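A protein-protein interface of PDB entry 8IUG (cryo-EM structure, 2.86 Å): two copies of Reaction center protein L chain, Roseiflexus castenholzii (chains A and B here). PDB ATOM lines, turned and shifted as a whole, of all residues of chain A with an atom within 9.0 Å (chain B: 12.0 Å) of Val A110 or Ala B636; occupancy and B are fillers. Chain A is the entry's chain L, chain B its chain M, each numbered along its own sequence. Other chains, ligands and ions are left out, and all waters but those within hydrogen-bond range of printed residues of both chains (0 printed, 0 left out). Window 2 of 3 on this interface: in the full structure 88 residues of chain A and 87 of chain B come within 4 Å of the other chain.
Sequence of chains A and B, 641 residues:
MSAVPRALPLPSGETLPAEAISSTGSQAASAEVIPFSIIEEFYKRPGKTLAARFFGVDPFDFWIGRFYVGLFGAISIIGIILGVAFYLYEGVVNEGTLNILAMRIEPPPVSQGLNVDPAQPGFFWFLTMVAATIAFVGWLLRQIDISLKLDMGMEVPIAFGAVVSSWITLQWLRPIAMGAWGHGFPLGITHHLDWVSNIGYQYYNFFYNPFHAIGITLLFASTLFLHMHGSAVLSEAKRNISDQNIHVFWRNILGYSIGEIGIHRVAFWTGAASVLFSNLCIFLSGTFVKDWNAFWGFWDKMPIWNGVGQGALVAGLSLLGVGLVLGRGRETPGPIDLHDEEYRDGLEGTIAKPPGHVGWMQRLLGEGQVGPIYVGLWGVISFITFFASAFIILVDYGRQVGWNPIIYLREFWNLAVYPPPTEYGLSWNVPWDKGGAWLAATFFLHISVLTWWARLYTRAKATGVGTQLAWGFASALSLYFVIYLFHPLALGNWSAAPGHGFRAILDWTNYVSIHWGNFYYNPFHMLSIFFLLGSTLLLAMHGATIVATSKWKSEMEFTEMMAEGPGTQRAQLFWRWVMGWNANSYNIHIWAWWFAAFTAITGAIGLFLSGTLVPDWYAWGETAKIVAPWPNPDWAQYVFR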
ATOM      1  N   PRO A 107     -27.671  21.312  28.360  1.00  0.00           N
ATOM      2  CA  PRO A 107     -27.776  21.507  26.911  1.00  0.00           C
ATOM      3  C   PRO A 107     -29.190  21.266  26.415  1.00  0.00           C
ATOM      4  O   PRO A 107     -30.096  20.979  27.211  1.00  0.00           O
ATOM      5  CB  PRO A 107     -26.798  20.460  26.351  1.00  0.00           C
ATOM      6  CG  PRO A 107     -26.589  19.497  27.431  1.00  0.00           C
ATOM      7  CD  PRO A 107     -26.732  20.232  28.702  1.00  0.00           C
ATOM      8  N   PRO A 108     -29.435  21.400  25.112  1.00  0.00           N
ATOM      9  CA  PRO A 108     -30.735  21.014  24.558  1.00  0.00           C
ATOM     10  C   PRO A 108     -30.932  19.511  24.633  1.00  0.00           C
ATOM     11  O   PRO A 108     -29.967  18.758  24.822  1.00  0.00           O
ATOM     12  CB  PRO A 108     -30.651  21.485  23.101  1.00  0.00           C
ATOM     13  CG  PRO A 108     -29.628  22.525  23.094  1.00  0.00           C
ATOM     14  CD  PRO A 108     -28.630  22.139  24.123  1.00  0.00           C
ATOM     15  N   PRO A 109     -32.166  19.031  24.508  1.00  0.00           N
ATOM     16  CA  PRO A 109     -32.384  17.586  24.434  1.00  0.00           C
ATOM     17  C   PRO A 109     -31.855  17.013  23.128  1.00  0.00           C
ATOM     18  O   PRO A 109     -31.603  17.728  22.156  1.00  0.00           O
ATOM     19  CB  PRO A 109     -33.906  17.451  24.531  1.00  0.00           C
ATOM     20  CG  PRO A 109     -34.426  18.756  24.096  1.00  0.00           C
ATOM     21  CD  PRO A 109     -33.435  19.773  24.541  1.00  0.00           C
ATOM     22  N   VAL A 110     -31.668  15.692  23.119  1.00  0.00           N
ATOM     23  CA  VAL A 110     -31.105  15.029  21.947  1.00  0.00           C
ATOM     24  C   VAL A 110     -32.080  14.954  20.785  1.00  0.00           C
ATOM     25  O   VAL A 110     -31.682  14.571  19.680  1.00  0.00           O
ATOM     26  CB  VAL A 110     -30.607  13.612  22.299  1.00  0.00           C
ATOM     27  CG1 VAL A 110     -29.546  13.674  23.370  1.00  0.00           C
ATOM     28  CG2 VAL A 110     -31.755  12.737  22.740  1.00  0.00           C
ATOM     29  N   SER A 111     -33.347  15.303  21.000  1.00  0.00           N
ATOM     30  CA  SER A 111     -34.323  15.326  19.920  1.00  0.00           C
ATOM     31  C   SER A 111     -34.196  16.558  19.039  1.00  0.00           C
ATOM     32  O   SER A 111     -34.784  16.587  17.954  1.00  0.00           O
ATOM     33  CB  SER A 111     -35.739  15.254  20.489  1.00  0.00           C
ATOM     34  OG  SER A 111     -36.012  16.369  21.314  1.00  0.00           O
ATOM     35  N   GLN A 112     -33.455  17.571  19.478  1.00  0.00           N
ATOM     36  CA  GLN A 112     -33.238  18.773  18.688  1.00  0.00           C
ATOM     37  C   GLN A 112     -32.116  18.614  17.672  1.00  0.00           C
ATOM     38  O   GLN A 112     -31.990  19.453  16.777  1.00  0.00           O
ATOM     39  CB  GLN A 112     -32.944  19.950  19.623  1.00  0.00           C
ATOM     40  CG  GLN A 112     -33.113  21.317  18.992  1.00  0.00           C
ATOM     41  CD  GLN A 112     -33.051  22.439  20.004  1.00  0.00           C
ATOM     42  OE1 GLN A 112     -33.920  22.562  20.862  1.00  0.00           O
ATOM     43  NE2 GLN A 112     -32.019  23.262  19.910  1.00  0.00           N
ATOM     44  N   GLY A 113     -31.312  17.557  17.775  1.00  0.00           N
ATOM     45  CA  GLY A 113     -30.208  17.369  16.860  1.00  0.00           C
ATOM     46  C   GLY A 113     -29.123  18.408  17.073  1.00  0.00           C
ATOM     47  O   GLY A 113     -28.880  18.882  18.185  1.00  0.00           O
ATOM     48  N   LEU A 114     -28.457  18.769  15.976  1.00  0.00           N
ATOM     49  CA  LEU A 114     -27.409  19.780  15.987  1.00  0.00           C
ATOM     50  C   LEU A 114     -27.935  21.163  15.635  1.00  0.00           C
ATOM     51  O   LEU A 114     -27.203  21.972  15.051  1.00  0.00           O
ATOM     52  CB  LEU A 114     -26.278  19.375  15.041  1.00  0.00           C
ATOM     53  CG  LEU A 114     -25.383  18.216  15.485  1.00  0.00           C
ATOM     54  CD1 LEU A 114     -24.589  17.686  14.321  1.00  0.00           C
ATOM     55  CD2 LEU A 114     -24.454  18.647  16.592  1.00  0.00           C
ATOM     56  N   ASN A 115     -29.187  21.452  15.971  1.00  0.00           N
ATOM     57  CA  ASN A 115     -29.811  22.741  15.720  1.00  0.00           C
ATOM     58  C   ASN A 115     -29.755  23.618  16.963  1.00  0.00           C
ATOM     59  O   ASN A 115     -29.840  23.133  18.093  1.00  0.00           O
ATOM     60  CB  ASN A 115     -31.268  22.566  15.292  1.00  0.00           C
ATOM     61  CG  ASN A 115     -31.408  21.821  13.988  1.00  0.00           C
ATOM     62  OD1 ASN A 115     -30.703  22.098  13.022  1.00  0.00           O
ATOM     63  ND2 ASN A 115     -32.325  20.867  13.951  1.00  0.00           N
ATOM     64  N   PRO A 121     -35.027  25.897  25.339  1.00  0.00           N
ATOM     65  CA  PRO A 121     -34.025  25.614  26.376  1.00  0.00           C
ATOM     66  C   PRO A 121     -32.679  25.070  25.860  1.00  0.00           C
ATOM     67  O   PRO A 121     -32.688  24.342  24.898  1.00  0.00           O
ATOM     68  CB  PRO A 121     -34.794  24.603  27.232  1.00  0.00           C
ATOM     69  CG  PRO A 121     -36.232  24.995  27.078  1.00  0.00           C
ATOM     70  CD  PRO A 121     -36.324  25.267  25.599  1.00  0.00           C
ATOM     71  N   PRO A 175     -20.037  15.145  20.744  1.00  0.00           N
ATOM     72  CA  PRO A 175     -21.424  15.494  20.394  1.00  0.00           C
ATOM     73  C   PRO A 175     -21.708  15.530  18.901  1.00  0.00           C
ATOM     74  O   PRO A 175     -22.799  15.134  18.483  1.00  0.00           O
ATOM     75  CB  PRO A 175     -21.596  16.874  21.035  1.00  0.00           C
ATOM     76  CG  PRO A 175     -20.705  16.846  22.183  1.00  0.00           C
ATOM     77  CD  PRO A 175     -19.498  16.079  21.748  1.00  0.00           C
ATOM     78  N   MET A 178     -21.710  11.778  17.661  1.00  0.00           N
ATOM     79  CA  MET A 178     -22.908  11.098  18.144  1.00  0.00           C
ATOM     80  C   MET A 178     -24.160  11.621  17.452  1.00  0.00           C
ATOM     81  O   MET A 178     -25.056  10.842  17.113  1.00  0.00           O
ATOM     82  CB  MET A 178     -23.030  11.252  19.658  1.00  0.00           C
ATOM     83  CG  MET A 178     -21.890  10.649  20.464  1.00  0.00           C
ATOM     84  SD  MET A 178     -22.071   8.906  20.819  1.00  0.00           S
ATOM     85  CE  MET A 178     -23.350   8.937  22.054  1.00  0.00           C
ATOM     86  N   GLY A 179     -24.254  12.932  17.249  1.00  0.00           N
ATOM     87  CA  GLY A 179     -25.299  13.479  16.407  1.00  0.00           C
ATOM     88  C   GLY A 179     -26.185  14.541  17.021  1.00  0.00           C
ATOM     89  O   GLY A 179     -27.184  14.925  16.410  1.00  0.00           O
ATOM     90  N   ALA A 180     -25.850  15.029  18.216  1.00  0.00           N
ATOM     91  CA  ALA A 180     -26.673  16.026  18.884  1.00  0.00           C
ATOM     92  C   ALA A 180     -25.826  16.822  19.861  1.00  0.00           C
ATOM     93  O   ALA A 180     -24.850  16.311  20.411  1.00  0.00           O
ATOM     94  CB  ALA A 180     -27.847  15.380  19.618  1.00  0.00           C
ATOM     95  N   TRP A 181     -26.215  18.083  20.076  1.00  0.00           N
ATOM     96  CA  TRP A 181     -25.606  18.913  21.111  1.00  0.00           C
ATOM     97  C   TRP A 181     -25.987  18.468  22.513  1.00  0.00           C
ATOM     98  O   TRP A 181     -25.336  18.883  23.474  1.00  0.00           O
ATOM     99  CB  TRP A 181     -26.000  20.384  20.945  1.00  0.00           C
ATOM    100  CG  TRP A 181     -25.426  21.081  19.750  1.00  0.00           C
ATOM    101  CD1 TRP A 181     -26.119  21.737  18.782  1.00  0.00           C
ATOM    102  CD2 TRP A 181     -24.041  21.202  19.404  1.00  0.00           C
ATOM    103  NE1 TRP A 181     -25.258  22.256  17.851  1.00  0.00           N
ATOM    104  CE2 TRP A 181     -23.975  21.938  18.208  1.00  0.00           C
ATOM    105  CE3 TRP A 181     -22.852  20.753  19.985  1.00  0.00           C
ATOM    106  CZ2 TRP A 181     -22.772  22.238  17.586  1.00  0.00           C
ATOM    107  CZ3 TRP A 181     -21.660  21.052  19.365  1.00  0.00           C
ATOM    108  CH2 TRP A 181     -21.627  21.788  18.179  1.00  0.00           C
ATOM    109  N   GLY A 182     -27.020  17.644  22.653  1.00  0.00           N
ATOM    110  CA  GLY A 182     -27.436  17.117  23.931  1.00  0.00           C
ATOM    111  C   GLY A 182     -26.593  15.986  24.456  1.00  0.00           C
ATOM    112  O   GLY A 182     -26.969  15.358  25.446  1.00  0.00           O
ATOM    113  N   HIS A 183     -25.466  15.696  23.810  1.00  0.00           N
ATOM    114  CA  HIS A 183     -24.506  14.707  24.272  1.00  0.00           C
ATOM    115  C   HIS A 183     -23.326  15.335  24.999  1.00  0.00           C
ATOM    116  O   HIS A 183     -22.346  14.640  25.280  1.00  0.00           O
ATOM    117  CB  HIS A 183     -24.003  13.864  23.096  1.00  0.00           C
ATOM    118  CG  HIS A 183     -25.037  12.952  22.512  1.00  0.00           C
ATOM    119  ND1 HIS A 183     -25.595  11.910  23.217  1.00  0.00           N
ATOM    120  CD2 HIS A 183     -25.600  12.918  21.283  1.00  0.00           C
ATOM    121  CE1 HIS A 183     -26.467  11.280  22.453  1.00  0.00           C
ATOM    122  NE2 HIS A 183     -26.488  11.871  21.273  1.00  0.00           N
ATOM    123  N   GLY A 184     -23.387  16.638  25.295  1.00  0.00           N
ATOM    124  CA  GLY A 184     -22.345  17.293  26.058  1.00  0.00           C
ATOM    125  C   GLY A 184     -22.673  17.369  27.534  1.00  0.00           C
ATOM    126  O   GLY A 184     -23.803  17.138  27.952  1.00  0.00           O
ATOM    127  N   TRP A 195     -23.644  13.703  35.236  1.00  0.00           N
ATOM    128  CA  TRP A 195     -23.368  13.280  33.870  1.00  0.00           C
ATOM    129  C   TRP A 195     -22.236  12.268  33.839  1.00  0.00           C
ATOM    130  O   TRP A 195     -22.324  11.252  33.140  1.00  0.00           O
ATOM    131  CB  TRP A 195     -23.030  14.494  33.003  1.00  0.00           C
ATOM    132  CG  TRP A 195     -22.842  14.194  31.534  1.00  0.00           C
ATOM    133  CD1 TRP A 195     -23.810  14.152  30.580  1.00  0.00           C
ATOM    134  CD2 TRP A 195     -21.607  13.914  30.861  1.00  0.00           C
ATOM    135  NE1 TRP A 195     -23.261  13.860  29.359  1.00  0.00           N
ATOM    136  CE2 TRP A 195     -21.910  13.709  29.505  1.00  0.00           C
ATOM    137  CE3 TRP A 195     -20.276  13.812  31.276  1.00  0.00           C
ATOM    138  CZ2 TRP A 195     -20.935  13.407  28.564  1.00  0.00           C
ATOM    139  CZ3 TRP A 195     -19.313  13.515  30.341  1.00  0.00           C
ATOM    140  CH2 TRP A 195     -19.646  13.318  29.000  1.00  0.00           C
ATOM    141  N   GLN A 202     -23.580   3.810  31.929  1.00  0.00           N
ATOM    142  CA  GLN A 202     -24.223   3.373  30.692  1.00  0.00           C
ATOM    143  C   GLN A 202     -23.325   2.431  29.901  1.00  0.00           C
ATOM    144  O   GLN A 202     -23.808   1.479  29.279  1.00  0.00           O
ATOM    145  CB  GLN A 202     -24.601   4.580  29.839  1.00  0.00           C
ATOM    146  CG  GLN A 202     -25.267   4.214  28.532  1.00  0.00           C
ATOM    147  CD  GLN A 202     -25.556   5.411  27.671  1.00  0.00           C
ATOM    148  OE1 GLN A 202     -25.094   6.512  27.946  1.00  0.00           O
ATOM    149  NE2 GLN A 202     -26.324   5.206  26.615  1.00  0.00           N
ATOM    150  N   TRP B 630     -33.354  18.364  39.610  1.00  0.00           N
ATOM    151  CA  TRP B 630     -33.510  17.508  38.433  1.00  0.00           C
ATOM    152  C   TRP B 630     -34.877  16.831  38.384  1.00  0.00           C
ATOM    153  O   TRP B 630     -34.966  15.611  38.564  1.00  0.00           O
ATOM    154  CB  TRP B 630     -32.410  16.445  38.397  1.00  0.00           C
ATOM    155  CG  TRP B 630     -31.977  16.064  37.022  1.00  0.00           C
ATOM    156  CD1 TRP B 630     -32.399  16.611  35.851  1.00  0.00           C
ATOM    157  CD2 TRP B 630     -31.027  15.053  36.674  1.00  0.00           C
ATOM    158  NE1 TRP B 630     -31.773  16.002  34.795  1.00  0.00           N
ATOM    159  CE2 TRP B 630     -30.923  15.043  35.275  1.00  0.00           C
ATOM    160  CE3 TRP B 630     -30.252  14.156  37.412  1.00  0.00           C
ATOM    161  CZ2 TRP B 630     -30.079  14.173  34.601  1.00  0.00           C
ATOM    162  CZ3 TRP B 630     -29.415  13.299  36.740  1.00  0.00           C
ATOM    163  CH2 TRP B 630     -29.334  13.311  35.352  1.00  0.00           C
ATOM    164  N   ASN B 632     -37.246  16.692  35.754  1.00  0.00           N
ATOM    165  CA  ASN B 632     -37.634  16.125  34.459  1.00  0.00           C
ATOM    166  C   ASN B 632     -36.390  15.804  33.643  1.00  0.00           C
ATOM    167  O   ASN B 632     -36.018  16.565  32.742  1.00  0.00           O
ATOM    168  CB  ASN B 632     -38.542  17.082  33.686  1.00  0.00           C
ATOM    169  CG  ASN B 632     -39.930  17.186  34.282  1.00  0.00           C
ATOM    170  OD1 ASN B 632     -40.534  16.183  34.659  1.00  0.00           O
ATOM    171  ND2 ASN B 632     -40.445  18.406  34.369  1.00  0.00           N
ATOM    172  N   PRO B 633     -35.723  14.689  33.930  1.00  0.00           N
ATOM    173  CA  PRO B 633     -34.545  14.313  33.142  1.00  0.00           C
ATOM    174  C   PRO B 633     -34.904  13.953  31.709  1.00  0.00           C
ATOM    175  O   PRO B 633     -35.990  13.447  31.420  1.00  0.00           O
ATOM    176  CB  PRO B 633     -33.991  13.098  33.890  1.00  0.00           C
ATOM    177  CG  PRO B 633     -34.574  13.181  35.248  1.00  0.00           C
ATOM    178  CD  PRO B 633     -35.925  13.779  35.067  1.00  0.00           C
ATOM    179  N   ASP B 634     -33.965  14.222  30.806  1.00  0.00           N
ATOM    180  CA  ASP B 634     -34.064  13.814  29.405  1.00  0.00           C
ATOM    181  C   ASP B 634     -33.284  12.511  29.268  1.00  0.00           C
ATOM    182  O   ASP B 634     -32.076  12.509  29.031  1.00  0.00           O
ATOM    183  CB  ASP B 634     -33.532  14.906  28.481  1.00  0.00           C
ATOM    184  CG  ASP B 634     -33.316  14.422  27.061  1.00  0.00           C
ATOM    185  OD1 ASP B 634     -34.307  14.075  26.388  1.00  0.00           O
ATOM    186  OD2 ASP B 634     -32.152  14.400  26.614  1.00  0.00           O
ATOM    187  N   TRP B 635     -33.982  11.391  29.429  1.00  0.00           N
ATOM    188  CA  TRP B 635     -33.326  10.096  29.524  1.00  0.00           C
ATOM    189  C   TRP B 635     -33.083   9.443  28.170  1.00  0.00           C
ATOM    190  O   TRP B 635     -32.446   8.387  28.116  1.00  0.00           O
ATOM    191  CB  TRP B 635     -34.137   9.156  30.421  1.00  0.00           C
ATOM    192  CG  TRP B 635     -33.260   8.325  31.289  1.00  0.00           C
ATOM    193  CD1 TRP B 635     -33.052   6.983  31.207  1.00  0.00           C
ATOM    194  CD2 TRP B 635     -32.436   8.794  32.358  1.00  0.00           C
ATOM    195  NE1 TRP B 635     -32.161   6.584  32.166  1.00  0.00           N
ATOM    196  CE2 TRP B 635     -31.764   7.680  32.885  1.00  0.00           C
ATOM    197  CE3 TRP B 635     -32.205  10.051  32.925  1.00  0.00           C
ATOM    198  CZ2 TRP B 635     -30.881   7.784  33.947  1.00  0.00           C
ATOM    199  CZ3 TRP B 635     -31.331  10.150  33.974  1.00  0.00           C
ATOM    200  CH2 TRP B 635     -30.679   9.026  34.476  1.00  0.00           C
ATOM    201  N   ALA B 636     -33.538  10.057  27.076  1.00  0.00           N
ATOM    202  CA  ALA B 636     -33.271   9.508  25.753  1.00  0.00           C
ATOM    203  C   ALA B 636     -31.786   9.488  25.434  1.00  0.00           C
ATOM    204  O   ALA B 636     -31.376   8.805  24.493  1.00  0.00           O
ATOM    205  CB  ALA B 636     -34.017  10.307  24.689  1.00  0.00           C
ATOM    206  N   GLN B 637     -30.975  10.226  26.193  1.00  0.00           N
ATOM    207  CA  GLN B 637     -29.532  10.174  26.009  1.00  0.00           C
ATOM    208  C   GLN B 637     -28.940   8.878  26.544  1.00  0.00           C
ATOM    209  O   GLN B 637     -27.924   8.405  26.024  1.00  0.00           O
ATOM    210  CB  GLN B 637     -28.876  11.371  26.692  1.00  0.00           C
ATOM    211  CG  GLN B 637     -27.374  11.414  26.540  1.00  0.00           C
ATOM    212  CD  GLN B 637     -26.726  12.473  27.388  1.00  0.00           C
ATOM    213  OE1 GLN B 637     -25.510  12.627  27.380  1.00  0.00           O
ATOM    214  NE2 GLN B 637     -27.533  13.211  28.126  1.00  0.00           N
ATOM    215  N   TYR B 638     -29.556   8.282  27.566  1.00  0.00           N
ATOM    216  CA  TYR B 638     -28.941   7.185  28.299  1.00  0.00           C
ATOM    217  C   TYR B 638     -29.512   5.823  27.929  1.00  0.00           C
ATOM    218  O   TYR B 638     -29.340   4.865  28.686  1.00  0.00           O
ATOM    219  CB  TYR B 638     -29.072   7.415  29.803  1.00  0.00           C
ATOM    220  CG  TYR B 638     -28.436   8.693  30.290  1.00  0.00           C
ATOM    221  CD1 TYR B 638     -27.062   8.859  30.267  1.00  0.00           C
ATOM    222  CD2 TYR B 638     -29.210   9.729  30.780  1.00  0.00           C
ATOM    223  CE1 TYR B 638     -26.480  10.023  30.711  1.00  0.00           C
ATOM    224  CE2 TYR B 638     -28.637  10.890  31.232  1.00  0.00           C
ATOM    225  CZ  TYR B 638     -27.273  11.032  31.197  1.00  0.00           C
ATOM    226  OH  TYR B 638     -26.702  12.195  31.647  1.00  0.00           O
ATOM    227  N   VAL B 639     -30.176   5.711  26.785  1.00  0.00           N
ATOM    228  CA  VAL B 639     -30.774   4.460  26.335  1.00  0.00           C
ATOM    229  C   VAL B 639     -30.367   4.220  24.888  1.00  0.00           C
ATOM    230  O   VAL B 639     -30.435   5.135  24.062  1.00  0.00           O
ATOM    231  CB  VAL B 639     -32.308   4.481  26.478  1.00  0.00           C
ATOM    232  CG1 VAL B 639     -32.925   3.254  25.841  1.00  0.00           C
ATOM    233  CG2 VAL B 639     -32.698   4.565  27.940  1.00  0.00           C
ATOM    234  N   PHE B 640     -29.931   3.000  24.588  1.00  0.00           N
ATOM    235  CA  PHE B 640     -29.639   2.602  23.216  1.00  0.00           C
ATOM    236  C   PHE B 640     -30.931   2.258  22.490  1.00  0.00           C
ATOM    237  O   PHE B 640     -31.092   2.554  21.309  1.00  0.00           O
ATOM    238  CB  PHE B 640     -28.690   1.403  23.174  1.00  0.00           C
ATOM    239  CG  PHE B 640     -27.419   1.596  23.947  1.00  0.00           C
ATOM    240  CD1 PHE B 640     -26.445   2.467  23.502  1.00  0.00           C
ATOM    241  CD2 PHE B 640     -27.189   0.885  25.106  1.00  0.00           C
ATOM    242  CE1 PHE B 640     -25.279   2.636  24.213  1.00  0.00           C
ATOM    243  CE2 PHE B 640     -26.025   1.052  25.814  1.00  0.00           C
ATOM    244  CZ  PHE B 640     -25.071   1.927  25.370  1.00  0.00           C
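The side-chain amide nitrogen (NE2) of Gln B637 is in hydrogen-bond range of the backbone carbonyl oxygen (O) of Gly A182, 3.5 Å away.
The indole nitrogen of Trp A195 sits at hydrogen-bond distance from the side-chain amide oxygen of Gln B637 (3.2 Å).
Asp B634 touches Pro A109.
Val A110 touches Asp B634.
CB of Ala B636 touches CG2 of Val A110, 3.8 Å away.
His A183 touches Gln B637 (ND1 to CG, 3.8 Å).
CD1 of Trp A195 touches OH of Tyr B638, at 3.7 Å.
Gln A202 touches Gln B637.
Tyr B638 touches Gln A202 (C to NE2, 3.5 Å).
Val B639 touches Gln A202.
NE2 of Gln A202 touches CE1 of Phe B640, 3.7 Å away.
Of chain B, only Asp B634 (3.8 Å) and Ala B636 (3.8 Å) come within 4 Å of Val A110.
Of chain A, only Val A110 comes within 4 Å of Ala B636.
No residue of chain B comes within 4 Å of Pro A108.
Of chain B, only Asp B634 comes within 4 Å of Pro A109.
No residue of chain B comes within 4 Å of Ser A111.
No residue of chain B comes within 4 Å of Gly A113.
No residue of chain B comes within 4 Å of Ala A180.
Of the printed residues of chain B, His A183 touches Gln B637.
Of the printed residues of chain A, Tyr B638 touches Trp A195 and Gln A202.
Printed residues of chain B within 4 Å of Gln A202: Gln B637 (3.6 Å), Tyr B638 (3.5 Å), Val B639 (3.9 Å) and Phe B640 (3.7 Å).
Of the printed residues of chain A, Val B639 touches Gln A202 (3.9 Å).
Printed residues of chain A within 4 Å of Gln B637: Gly A182, His A183, Trp A195 and Gln A202.
Leu A114 touches none of the printed residues of chain B.
The nearest residue of chain B that does not touch Val A110 is Gln B637 (4.1 Å).
The nearest residue of chain A that does not touch Ala B636 is His A183 (5.9 Å).
The nearest printed residue of chain B that does not touch Trp A195 is Trp B630 (5.7 Å).
Hydrophobic or aromatic side chains of chain A within 4 Å of the printed part of chain B: Pro A109, Val A110, His A183 and Trp A195.
Of the 10 printed residues of chain B, 6 touch a printed residue of chain A.
Printed residues of chain B that touch a printed residue of chain A: Asp B634, Ala B636, Gln B637, Tyr B638, Val B639 and Phe B640.
Hydrophobic or aromatic side chains of chain B that line the printed part of chain A: Ala B636, Tyr B638 and Phe B640.
Among the printed residues, no Asp or Glu carboxylate lies within 4 Å of a Lys or Arg side-chain nitrogen of the other chain.
No position is printed for both chains.
Of the 11 pairs that touch across the chains among the printed residues, none has its exchanged pair printed and touching as well.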
